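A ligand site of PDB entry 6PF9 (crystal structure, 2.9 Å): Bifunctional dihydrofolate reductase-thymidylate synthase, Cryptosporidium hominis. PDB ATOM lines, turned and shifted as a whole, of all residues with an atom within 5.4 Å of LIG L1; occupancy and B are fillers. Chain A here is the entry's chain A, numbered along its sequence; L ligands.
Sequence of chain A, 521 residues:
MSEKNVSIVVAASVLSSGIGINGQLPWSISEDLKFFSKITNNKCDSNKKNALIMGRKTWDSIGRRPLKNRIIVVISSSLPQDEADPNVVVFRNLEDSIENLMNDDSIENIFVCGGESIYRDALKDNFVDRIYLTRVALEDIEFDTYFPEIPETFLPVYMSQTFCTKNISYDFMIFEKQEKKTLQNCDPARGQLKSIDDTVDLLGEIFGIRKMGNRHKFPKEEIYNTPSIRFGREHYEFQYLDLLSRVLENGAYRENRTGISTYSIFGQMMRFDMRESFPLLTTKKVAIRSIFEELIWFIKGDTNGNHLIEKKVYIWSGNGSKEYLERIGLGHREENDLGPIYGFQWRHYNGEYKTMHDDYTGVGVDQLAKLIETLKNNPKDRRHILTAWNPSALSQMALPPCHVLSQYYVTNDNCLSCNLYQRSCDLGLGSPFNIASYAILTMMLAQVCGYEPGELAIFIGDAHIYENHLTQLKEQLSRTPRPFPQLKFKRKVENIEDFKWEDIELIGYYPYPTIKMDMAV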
ATOM      1  N   VAL A   9     -13.535  -8.019   4.370  1.00  0.00           N
ATOM      2  CA  VAL A   9     -12.155  -8.007   4.840  1.00  0.00           C
ATOM      3  C   VAL A   9     -11.302  -7.383   3.753  1.00  0.00           C
ATOM      4  O   VAL A   9     -11.389  -7.784   2.586  1.00  0.00           O
ATOM      5  CB  VAL A   9     -11.657  -9.428   5.186  1.00  0.00           C
ATOM      6  CG1 VAL A   9     -10.335  -9.358   5.936  1.00  0.00           C
ATOM      7  CG2 VAL A   9     -12.712 -10.181   5.986  1.00  0.00           C
ATOM      8  N   VAL A  10     -10.493  -6.393   4.121  1.00  0.00           N
ATOM      9  CA  VAL A  10      -9.723  -5.635   3.142  1.00  0.00           C
ATOM     10  C   VAL A  10      -8.538  -4.999   3.844  1.00  0.00           C
ATOM     11  O   VAL A  10      -8.586  -4.705   5.046  1.00  0.00           O
ATOM     12  CB  VAL A  10     -10.611  -4.581   2.433  1.00  0.00           C
ATOM     13  CG1 VAL A  10     -11.131  -3.553   3.424  1.00  0.00           C
ATOM     14  CG2 VAL A  10      -9.854  -3.901   1.293  1.00  0.00           C
ATOM     15  N   ALA A  11      -7.452  -4.797   3.089  1.00  0.00           N
ATOM     16  CA  ALA A  11      -6.284  -4.046   3.545  1.00  0.00           C
ATOM     17  C   ALA A  11      -6.019  -2.941   2.536  1.00  0.00           C
ATOM     18  O   ALA A  11      -5.586  -3.214   1.407  1.00  0.00           O
ATOM     19  CB  ALA A  11      -5.061  -4.956   3.690  1.00  0.00           C
ATOM     20  N   LEU A  25      -0.467  -7.409  -4.460  1.00  0.00           N
ATOM     21  CA  LEU A  25      -0.527  -6.446  -3.368  1.00  0.00           C
ATOM     22  C   LEU A  25       0.656  -5.493  -3.430  1.00  0.00           C
ATOM     23  O   LEU A  25       1.764  -5.875  -3.822  1.00  0.00           O
ATOM     24  CB  LEU A  25      -0.534  -7.168  -2.024  1.00  0.00           C
ATOM     25  CG  LEU A  25      -1.603  -8.232  -1.817  1.00  0.00           C
ATOM     26  CD1 LEU A  25      -1.370  -8.967  -0.504  1.00  0.00           C
ATOM     27  CD2 LEU A  25      -2.991  -7.618  -1.852  1.00  0.00           C
ATOM     28  N   SER A  30       3.337  -9.951   6.716  1.00  0.00           N
ATOM     29  CA  SER A  30       3.022 -11.315   7.122  1.00  0.00           C
ATOM     30  C   SER A  30       1.895 -11.361   8.154  1.00  0.00           C
ATOM     31  O   SER A  30       0.995 -12.207   8.051  1.00  0.00           O
ATOM     32  CB  SER A  30       4.267 -11.995   7.677  1.00  0.00           C
ATOM     33  OG  SER A  30       3.970 -13.295   8.159  1.00  0.00           O
ATOM     34  N   ASP A  32      -0.553  -9.401   8.558  1.00  0.00           N
ATOM     35  CA  ASP A  32      -1.855  -9.101   7.961  1.00  0.00           C
ATOM     36  C   ASP A  32      -2.475 -10.352   7.341  1.00  0.00           C
ATOM     37  O   ASP A  32      -3.684 -10.586   7.468  1.00  0.00           O
ATOM     38  CB  ASP A  32      -1.712  -7.999   6.923  1.00  0.00           C
ATOM     39  CG  ASP A  32      -3.005  -7.709   6.194  1.00  0.00           C
ATOM     40  OD1 ASP A  32      -4.037  -7.461   6.868  1.00  0.00           O
ATOM     41  OD2 ASP A  32      -3.001  -7.727   4.947  1.00  0.00           O
ATOM     42  N   LEU A  33      -1.658 -11.171   6.655  1.00  0.00           N
ATOM     43  CA  LEU A  33      -2.183 -12.409   6.083  1.00  0.00           C
ATOM     44  C   LEU A  33      -2.638 -13.366   7.173  1.00  0.00           C
ATOM     45  O   LEU A  33      -3.613 -14.097   7.002  1.00  0.00           O
ATOM     46  CB  LEU A  33      -1.115 -13.065   5.202  1.00  0.00           C
ATOM     47  CG  LEU A  33      -0.750 -12.326   3.918  1.00  0.00           C
ATOM     48  CD1 LEU A  33       0.309 -13.095   3.130  1.00  0.00           C
ATOM     49  CD2 LEU A  33      -1.993 -12.106   3.070  1.00  0.00           C
ATOM     50  N   LYS A  34      -1.931 -13.385   8.312  1.00  0.00           N
ATOM     51  CA  LYS A  34      -2.366 -14.196   9.448  1.00  0.00           C
ATOM     52  C   LYS A  34      -3.697 -13.687  10.003  1.00  0.00           C
ATOM     53  O   LYS A  34      -4.553 -14.487  10.400  1.00  0.00           O
ATOM     54  CB  LYS A  34      -1.294 -14.216  10.526  1.00  0.00           C
ATOM     55  N   PHE A  35      -3.878 -12.371  10.026  1.00  0.00           N
ATOM     56  CA  PHE A  35      -5.157 -11.810  10.469  1.00  0.00           C
ATOM     57  C   PHE A  35      -6.290 -12.229   9.534  1.00  0.00           C
ATOM     58  O   PHE A  35      -7.376 -12.611   9.996  1.00  0.00           O
ATOM     59  CB  PHE A  35      -5.071 -10.286  10.563  1.00  0.00           C
ATOM     60  CG  PHE A  35      -6.375  -9.623  10.920  1.00  0.00           C
ATOM     61  CD1 PHE A  35      -6.853  -9.665  12.218  1.00  0.00           C
ATOM     62  CD2 PHE A  35      -7.108  -8.960   9.960  1.00  0.00           C
ATOM     63  CE1 PHE A  35      -8.056  -9.055  12.550  1.00  0.00           C
ATOM     64  CE2 PHE A  35      -8.306  -8.352  10.284  1.00  0.00           C
ATOM     65  CZ  PHE A  35      -8.784  -8.394  11.581  1.00  0.00           C
ATOM     66  N   PHE A  36      -6.060 -12.150   8.223  1.00  0.00           N
ATOM     67  CA  PHE A  36      -7.062 -12.594   7.271  1.00  0.00           C
ATOM     68  C   PHE A  36      -7.384 -14.079   7.470  1.00  0.00           C
ATOM     69  O   PHE A  36      -8.551 -14.480   7.395  1.00  0.00           O
ATOM     70  CB  PHE A  36      -6.588 -12.331   5.848  1.00  0.00           C
ATOM     71  CG  PHE A  36      -7.479 -12.933   4.785  1.00  0.00           C
ATOM     72  CD1 PHE A  36      -8.603 -12.254   4.354  1.00  0.00           C
ATOM     73  CD2 PHE A  36      -7.189 -14.157   4.229  1.00  0.00           C
ATOM     74  CE1 PHE A  36      -9.433 -12.798   3.391  1.00  0.00           C
ATOM     75  CE2 PHE A  36      -8.003 -14.707   3.265  1.00  0.00           C
ATOM     76  CZ  PHE A  36      -9.126 -14.028   2.834  1.00  0.00           C
ATOM     77  N   SER A  37      -6.358 -14.881   7.740  1.00  0.00           N
ATOM     78  CA  SER A  37      -6.578 -16.314   7.912  1.00  0.00           C
ATOM     79  C   SER A  37      -7.401 -16.610   9.156  1.00  0.00           C
ATOM     80  O   SER A  37      -8.283 -17.481   9.138  1.00  0.00           O
ATOM     81  CB  SER A  37      -5.237 -17.046   7.962  1.00  0.00           C
ATOM     82  OG  SER A  37      -5.424 -18.444   8.156  1.00  0.00           O
ATOM     83  N   THR A  40     -11.202 -15.148   8.897  1.00  0.00           N
ATOM     84  CA  THR A  40     -12.078 -15.884   7.991  1.00  0.00           C
ATOM     85  C   THR A  40     -12.313 -17.321   8.423  1.00  0.00           C
ATOM     86  O   THR A  40     -13.256 -17.952   7.932  1.00  0.00           O
ATOM     87  CB  THR A  40     -11.526 -15.860   6.564  1.00  0.00           C
ATOM     88  OG1 THR A  40     -10.183 -16.369   6.561  1.00  0.00           O
ATOM     89  CG2 THR A  40     -11.526 -14.441   6.011  1.00  0.00           C
ATOM     90  N   ASN A  41     -11.474 -17.860   9.306  1.00  0.00           N
ATOM     91  CA  ASN A  41     -11.684 -19.179   9.874  1.00  0.00           C
ATOM     92  C   ASN A  41     -12.447 -19.147  11.198  1.00  0.00           C
ATOM     93  O   ASN A  41     -12.797 -20.214  11.722  1.00  0.00           O
ATOM     94  CB  ASN A  41     -10.342 -19.896  10.083  1.00  0.00           C
ATOM     95  CG  ASN A  41      -9.860 -20.598   8.841  1.00  0.00           C
ATOM     96  OD1 ASN A  41     -10.648 -21.200   8.101  1.00  0.00           O
ATOM     97  ND2 ASN A  41      -8.561 -20.546   8.597  1.00  0.00           N
ATOM     98  N   THR A  58      -8.756 -11.605  -8.327  1.00  0.00           N
ATOM     99  CA  THR A  58      -8.239 -11.968  -7.009  1.00  0.00           C
ATOM    100  C   THR A  58      -8.014 -13.477  -6.928  1.00  0.00           C
ATOM    101  O   THR A  58      -7.036 -13.937  -6.326  1.00  0.00           O
ATOM    102  CB  THR A  58      -9.214 -11.510  -5.926  1.00  0.00           C
ATOM    103  OG1 THR A  58      -9.327 -10.078  -5.964  1.00  0.00           O
ATOM    104  CG2 THR A  58      -8.737 -11.932  -4.546  1.00  0.00           C
ATOM    105  N   SER A  61      -4.815 -14.096  -8.218  1.00  0.00           N
ATOM    106  CA  SER A  61      -3.738 -13.609  -7.365  1.00  0.00           C
ATOM    107  C   SER A  61      -3.292 -14.662  -6.347  1.00  0.00           C
ATOM    108  O   SER A  61      -2.112 -14.687  -5.963  1.00  0.00           O
ATOM    109  CB  SER A  61      -4.162 -12.336  -6.636  1.00  0.00           C
ATOM    110  OG  SER A  61      -4.428 -11.298  -7.565  1.00  0.00           O
ATOM    111  N   ILE A  62      -4.199 -15.516  -5.895  1.00  0.00           N
ATOM    112  CA  ILE A  62      -3.872 -16.519  -4.895  1.00  0.00           C
ATOM    113  C   ILE A  62      -3.515 -17.834  -5.579  1.00  0.00           C
ATOM    114  O   ILE A  62      -3.548 -18.905  -4.954  1.00  0.00           O
ATOM    115  CB  ILE A  62      -5.025 -16.715  -3.888  1.00  0.00           C
ATOM    116  CG1 ILE A  62      -6.269 -17.277  -4.581  1.00  0.00           C
ATOM    117  CG2 ILE A  62      -5.341 -15.407  -3.203  1.00  0.00           C
ATOM    118  CD1 ILE A  62      -7.417 -17.545  -3.634  1.00  0.00           C
ATOM    119  N   LEU A  67      -8.302 -22.400  -0.167  1.00  0.00           N
ATOM    120  CA  LEU A  67      -7.874 -22.053   1.173  1.00  0.00           C
ATOM    121  C   LEU A  67      -8.415 -23.082   2.154  1.00  0.00           C
ATOM    122  O   LEU A  67      -9.582 -23.483   2.079  1.00  0.00           O
ATOM    123  CB  LEU A  67      -8.349 -20.650   1.564  1.00  0.00           C
ATOM    124  CG  LEU A  67      -7.686 -19.497   0.804  1.00  0.00           C
ATOM    125  CD1 LEU A  67      -8.413 -18.190   1.048  1.00  0.00           C
ATOM    126  CD2 LEU A  67      -6.233 -19.365   1.191  1.00  0.00           C
ATOM    127  N   ARG A  70     -12.075 -23.649   4.240  1.00  0.00           N
ATOM    128  CA  ARG A  70     -12.972 -22.610   3.762  1.00  0.00           C
ATOM    129  C   ARG A  70     -13.396 -22.925   2.335  1.00  0.00           C
ATOM    130  O   ARG A  70     -12.723 -23.649   1.595  1.00  0.00           O
ATOM    131  CB  ARG A  70     -12.304 -21.223   3.818  1.00  0.00           C
ATOM    132  CG  ARG A  70     -12.273 -20.624   5.209  1.00  0.00           C
ATOM    133  CD  ARG A  70     -11.135 -19.638   5.336  1.00  0.00           C
ATOM    134  NE  ARG A  70      -9.838 -20.307   5.254  1.00  0.00           N
ATOM    135  CZ  ARG A  70      -8.668 -19.689   5.314  1.00  0.00           C
ATOM    136  NH1 ARG A  70      -8.613 -18.377   5.454  1.00  0.00           N
ATOM    137  NH2 ARG A  70      -7.546 -20.393   5.228  1.00  0.00           N
ATOM    138  N   CYS A 113     -13.984 -10.759   0.432  1.00  0.00           N
ATOM    139  CA  CYS A 113     -12.606 -10.317   0.285  1.00  0.00           C
ATOM    140  C   CYS A 113     -12.202 -10.279  -1.190  1.00  0.00           C
ATOM    141  O   CYS A 113     -11.200 -10.886  -1.573  1.00  0.00           O
ATOM    142  CB  CYS A 113     -11.670 -11.226   1.090  1.00  0.00           C
ATOM    143  SG  CYS A 113     -11.963 -12.986   0.815  1.00  0.00           S
ATOM    144  N   TYR A 119     -15.964  -5.241  -4.247  1.00  0.00           N
ATOM    145  CA  TYR A 119     -16.222  -4.376  -3.098  1.00  0.00           C
ATOM    146  C   TYR A 119     -17.281  -3.331  -3.421  1.00  0.00           C
ATOM    147  O   TYR A 119     -18.167  -3.053  -2.606  1.00  0.00           O
ATOM    148  CB  TYR A 119     -14.929  -3.686  -2.653  1.00  0.00           C
ATOM    149  CG  TYR A 119     -13.966  -4.563  -1.901  1.00  0.00           C
ATOM    150  CD1 TYR A 119     -14.424  -5.528  -1.006  1.00  0.00           C
ATOM    151  CD2 TYR A 119     -12.594  -4.413  -2.071  1.00  0.00           C
ATOM    152  CE1 TYR A 119     -13.527  -6.331  -0.318  1.00  0.00           C
ATOM    153  CE2 TYR A 119     -11.700  -5.208  -1.387  1.00  0.00           C
ATOM    154  CZ  TYR A 119     -12.173  -6.161  -0.504  1.00  0.00           C
ATOM    155  OH  TYR A 119     -11.279  -6.956   0.180  1.00  0.00           O
ATOM    156  N   TYR A 132     -13.817  -5.214   8.086  1.00  0.00           N
ATOM    157  CA  TYR A 132     -12.525  -5.386   8.739  1.00  0.00           C
ATOM    158  C   TYR A 132     -11.473  -4.695   7.882  1.00  0.00           C
ATOM    159  O   TYR A 132     -11.025  -5.245   6.875  1.00  0.00           O
ATOM    160  CB  TYR A 132     -12.195  -6.859   8.938  1.00  0.00           C
ATOM    161  CG  TYR A 132     -13.067  -7.585   9.946  1.00  0.00           C
ATOM    162  CD1 TYR A 132     -12.756  -7.579  11.307  1.00  0.00           C
ATOM    163  CD2 TYR A 132     -14.189  -8.305   9.543  1.00  0.00           C
ATOM    164  CE1 TYR A 132     -13.534  -8.246  12.236  1.00  0.00           C
ATOM    165  CE2 TYR A 132     -14.981  -8.975  10.453  1.00  0.00           C
ATOM    166  CZ  TYR A 132     -14.643  -8.942  11.798  1.00  0.00           C
ATOM    167  OH  TYR A 132     -15.429  -9.613  12.724  1.00  0.00           O
ATOM    168  N   THR A 134      -7.763  -2.944   7.276  1.00  0.00           N
ATOM    169  CA  THR A 134      -6.366  -2.941   7.688  1.00  0.00           C
ATOM    170  C   THR A 134      -5.692  -1.758   7.008  1.00  0.00           C
ATOM    171  O   THR A 134      -5.236  -1.850   5.870  1.00  0.00           O
ATOM    172  CB  THR A 134      -5.677  -4.254   7.333  1.00  0.00           C
ATOM    173  OG1 THR A 134      -6.434  -5.355   7.855  1.00  0.00           O
ATOM    174  CG2 THR A 134      -4.262  -4.294   7.915  1.00  0.00           C
HETATM  175  N1  LIG L   1      -5.379  -8.487   3.647  1.00  0.00           N
HETATM  176  C1  LIG L   1      -6.489  -8.134   4.335  1.00  0.00           C
HETATM  177  N2  LIG L   1      -6.344  -7.441   5.579  1.00  0.00           N
HETATM  178  N3  LIG L   1      -7.725  -8.416   3.892  1.00  0.00           N
HETATM  179  C2  LIG L   1      -7.907  -9.077   2.725  1.00  0.00           C
HETATM  180  N4  LIG L   1      -9.215  -9.379   2.248  1.00  0.00           N
HETATM  181  C3  LIG L   1      -6.772  -9.465   1.965  1.00  0.00           C
HETATM  182  N5  LIG L   1      -6.912 -10.126   0.786  1.00  0.00           N
HETATM  183  C4  LIG L   1      -5.797 -10.466   0.098  1.00  0.00           C
HETATM  184  C5  LIG L   1      -4.517 -10.170   0.561  1.00  0.00           C
HETATM  185  N6  LIG L   1      -4.398  -9.515   1.742  1.00  0.00           N
HETATM  186  C6  LIG L   1      -5.514  -9.151   2.460  1.00  0.00           C
HETATM  187  C7  LIG L   1      -5.960 -11.209  -1.213  1.00  0.00           C
HETATM  188  N7  LIG L   1      -4.868 -12.109  -1.523  1.00  0.00           N
HETATM  189  C8  LIG L   1      -4.066 -11.900  -2.710  1.00  0.00           C
HETATM  190  C9  LIG L   1      -3.919 -15.346   1.061  1.00  0.00           C
HETATM  191  C10 LIG L   1      -2.932 -14.708   0.321  1.00  0.00           C
HETATM  192  C11 LIG L   1      -3.256 -13.652  -0.516  1.00  0.00           C
HETATM  193  C12 LIG L   1      -4.570 -13.220  -0.629  1.00  0.00           C
HETATM  194  C13 LIG L   1      -5.566 -13.862   0.107  1.00  0.00           C
HETATM  195  C14 LIG L   1      -5.243 -14.924   0.956  1.00  0.00           C
HETATM  196  C15 LIG L   1      -3.547 -16.490   1.968  1.00  0.00           C
HETATM  197  O1  LIG L   1      -2.601 -17.202   1.662  1.00  0.00           O
HETATM  198  N8  LIG L   1      -4.256 -16.760   3.197  1.00  0.00           N
HETATM  199  C16 LIG L   1      -3.857 -17.865   4.039  1.00  0.00           C
HETATM  200  C17 LIG L   1      -5.063 -18.405   4.696  1.00  0.00           C
HETATM  201  O2  LIG L   1      -6.189 -17.921   4.403  1.00  0.00           O
HETATM  202  O3  LIG L   1      -4.967 -19.347   5.545  1.00  0.00           O
HETATM  203  C18 LIG L   1      -2.941 -17.347   5.101  1.00  0.00           C
HETATM  204  C19 LIG L   1      -1.464 -17.564   4.983  1.00  0.00           C
HETATM  205  C20 LIG L   1      -0.673 -17.368   6.241  1.00  0.00           C
HETATM  206  O4  LIG L   1      -1.164 -17.732   7.331  1.00  0.00           O
HETATM  207  O5  LIG L   1       0.294 -16.566   6.240  1.00  0.00           O
HETATM  208  P1  LG2 L   2     -11.441  -8.419  -8.951  1.00  0.00           P
HETATM  209  O1  LG2 L   2     -12.414  -7.448  -8.305  1.00  0.00           O
HETATM  210  O2  LG2 L   2     -10.743  -9.207  -7.874  1.00  0.00           O
HETATM  211  O3  LG2 L   2     -12.228  -9.389  -9.834  1.00  0.00           O
HETATM  212  C1  LG2 L   2     -12.582  -9.038 -11.142  1.00  0.00           C
HETATM  213  C2  LG2 L   2     -13.334 -10.039 -11.917  1.00  0.00           C
HETATM  214  O4  LG2 L   2     -14.521 -10.381 -11.228  1.00  0.00           O
HETATM  215  C3  LG2 L   2     -13.793  -9.537 -13.213  1.00  0.00           C
HETATM  216  O5  LG2 L   2     -12.813  -9.638 -14.183  1.00  0.00           O
HETATM  217  C4  LG2 L   2     -14.913 -10.402 -13.499  1.00  0.00           C
HETATM  218  O6  LG2 L   2     -14.477 -11.659 -13.946  1.00  0.00           O
HETATM  219  C5  LG2 L   2     -15.542 -10.585 -12.202  1.00  0.00           C
HETATM  220  N1  LG2 L   2     -16.601  -9.644 -12.036  1.00  0.00           N
HETATM  221  C6  LG2 L   2     -16.515  -8.421 -11.475  1.00  0.00           C
HETATM  222  N2  LG2 L   2     -17.726  -7.832 -11.490  1.00  0.00           N
HETATM  223  C7  LG2 L   2     -18.616  -8.698 -12.081  1.00  0.00           C
HETATM  224  C8  LG2 L   2     -20.006  -8.646 -12.375  1.00  0.00           C
HETATM  225  N3  LG2 L   2     -20.786  -7.427 -12.022  1.00  0.00           N
HETATM  226  N4  LG2 L   2     -20.608  -9.699 -12.988  1.00  0.00           N
HETATM  227  C9  LG2 L   2     -19.874 -10.801 -13.301  1.00  0.00           C
HETATM  228  N5  LG2 L   2     -18.570 -10.892 -13.043  1.00  0.00           N
HETATM  229  C10 LG2 L   2     -17.902  -9.847 -12.429  1.00  0.00           C
HETATM  230  O7  LG2 L   2     -10.366  -7.616  -9.812  1.00  0.00           O
HETATM  231  P2  LG2 L   2      -9.549  -6.392  -9.218  1.00  0.00           P
HETATM  232  O8  LG2 L   2      -8.522  -5.880 -10.242  1.00  0.00           O
HETATM  233  O9  LG2 L   2     -10.513  -5.266  -8.883  1.00  0.00           O
HETATM  234  O10 LG2 L   2      -8.755  -6.848  -7.881  1.00  0.00           O
HETATM  235  C11 LG2 L   2      -7.467  -7.395  -7.997  1.00  0.00           C
HETATM  236  C12 LG2 L   2      -6.373  -6.698  -7.336  1.00  0.00           C
HETATM  237  O11 LG2 L   2      -6.761  -6.313  -6.025  1.00  0.00           O
HETATM  238  C13 LG2 L   2      -5.199  -7.574  -7.178  1.00  0.00           C
HETATM  239  O12 LG2 L   2      -4.035  -6.809  -7.227  1.00  0.00           O
HETATM  240  C14 LG2 L   2      -5.346  -8.113  -5.873  1.00  0.00           C
HETATM  241  O13 LG2 L   2      -4.099  -8.503  -5.376  1.00  0.00           O
HETATM  242  C15 LG2 L   2      -5.904  -6.956  -5.130  1.00  0.00           C
HETATM  243  N6  LG2 L   2      -6.597  -7.385  -3.958  1.00  0.00           N
HETATM  244  C16 LG2 L   2      -6.327  -6.771  -2.791  1.00  0.00           C
HETATM  245  C17 LG2 L   2      -6.970  -7.151  -1.604  1.00  0.00           C
HETATM  246  C18 LG2 L   2      -6.626  -6.429  -0.318  1.00  0.00           C
HETATM  247  O14 LG2 L   2      -7.283  -6.676   0.712  1.00  0.00           O
HETATM  248  N7  LG2 L   2      -5.572  -5.454  -0.269  1.00  0.00           N
HETATM  249  C19 LG2 L   2      -7.922  -8.192  -1.630  1.00  0.00           C
HETATM  250  C20 LG2 L   2      -8.179  -8.807  -2.860  1.00  0.00           C
HETATM  251  C21 LG2 L   2      -7.517  -8.402  -4.007  1.00  0.00           C
HETATM  252  P3  LG2 L   2     -14.639 -12.087 -15.438  1.00  0.00           P
HETATM  253  O15 LG2 L   2     -14.059 -10.971 -16.338  1.00  0.00           O
HETATM  254  O16 LG2 L   2     -13.932 -13.348 -15.669  1.00  0.00           O
HETATM  255  O17 LG2 L   2     -16.089 -12.292 -15.759  1.00  0.00           O
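A nitrogen (N2) of LIG L1 sits at hydrogen-bond distance from the side-chain carboxylate (OD1) of Asp 32 (2.6 Å). An oxygen (O2) of LIG L1 lies within salt-bridge range of the guanidinium group (NH1) of Arg 70 (2.7 Å). The backbone carbonyl oxygen (O) of Val 9 sits at hydrogen-bond distance from a nitrogen (N4) of LIG L1, 2.7 Å away. O3 of LIG L1 sits at hydrogen-bond distance from OG of Ser 37 (2.8 Å). OG1 of Thr 134 sits at hydrogen-bond distance from N2 of LIG L1, at 3.1 Å. A nitrogen (N3) of LIG L1 is in hydrogen-bond range of the backbone NH (N) of Val 10 (3.4 Å). An oxygen (O14) of LG2 L2 sits at hydrogen-bond distance from the backbone NH of Ala 11 (3.0 Å). The backbone carbonyl oxygen (O) of Ala 11 lies within hydrogen-bond range of a nitrogen (N7) of LG2 L2 (2.8 Å). N of Thr 58 sits at hydrogen-bond distance from O2 of LG2 L2 (3.1 Å). The side-chain hydroxyl of Thr 58 lies within hydrogen-bond range of an oxygen (O2) of LG2 L2 (2.5 Å).
Ala 11 touches LIG L1. Leu 25 touches LIG L1. CD2 of Leu 33 touches N6 of LIG L1, at 3.8 Å. CE2 of Phe 36 touches C14 of LIG L1, 3.6 Å away. Ser 61 touches LIG L1. Ile 62 touches LIG L1. Leu 67 touches LIG L1 (CD2 to O2, 3.5 Å). Cys 113 touches LIG L1 (CB to N4, 3.3 Å). OH of Tyr 119 touches N4 of LIG L1, 3.8 Å away. Hydrophobic or aromatic side chains that line LIG L1: Val 9, Ala 11, Leu 25, Leu 33, Phe 36, Ile 62 and Leu 67. Along chain A the residues within 4 Å of LIG L1 span positions 9 to 134.
The side-chain carboxylate (OD1) of Asp 32 is in hydrogen-bond range of the side-chain hydroxyl (OG1) of Thr 134, at 3.3 Å. The guanidinium group of Arg 70 lies within hydrogen-bond range of the side-chain amide oxygen of Asn 41 (3.1 Å). OH of Tyr 119 lies within hydrogen-bond range of O of Val 9 (2.5 Å). O of Ser 37 sits at hydrogen-bond distance from OG1 of Thr 40, 3.4 Å away. The side-chain amide nitrogen of Asn 41 sits at hydrogen-bond distance from the backbone carbonyl oxygen of Ser 37 (3.1 Å). O of Val 10 sits at hydrogen-bond distance from N of Thr 134 (3.0 Å). The backbone NH (N) of Val 10 sits at hydrogen-bond distance from the backbone carbonyl oxygen (O) of Tyr 132 (3.0 Å). O of Phe 36 lies within hydrogen-bond range of OG1 of Thr 40 (2.6 Å).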
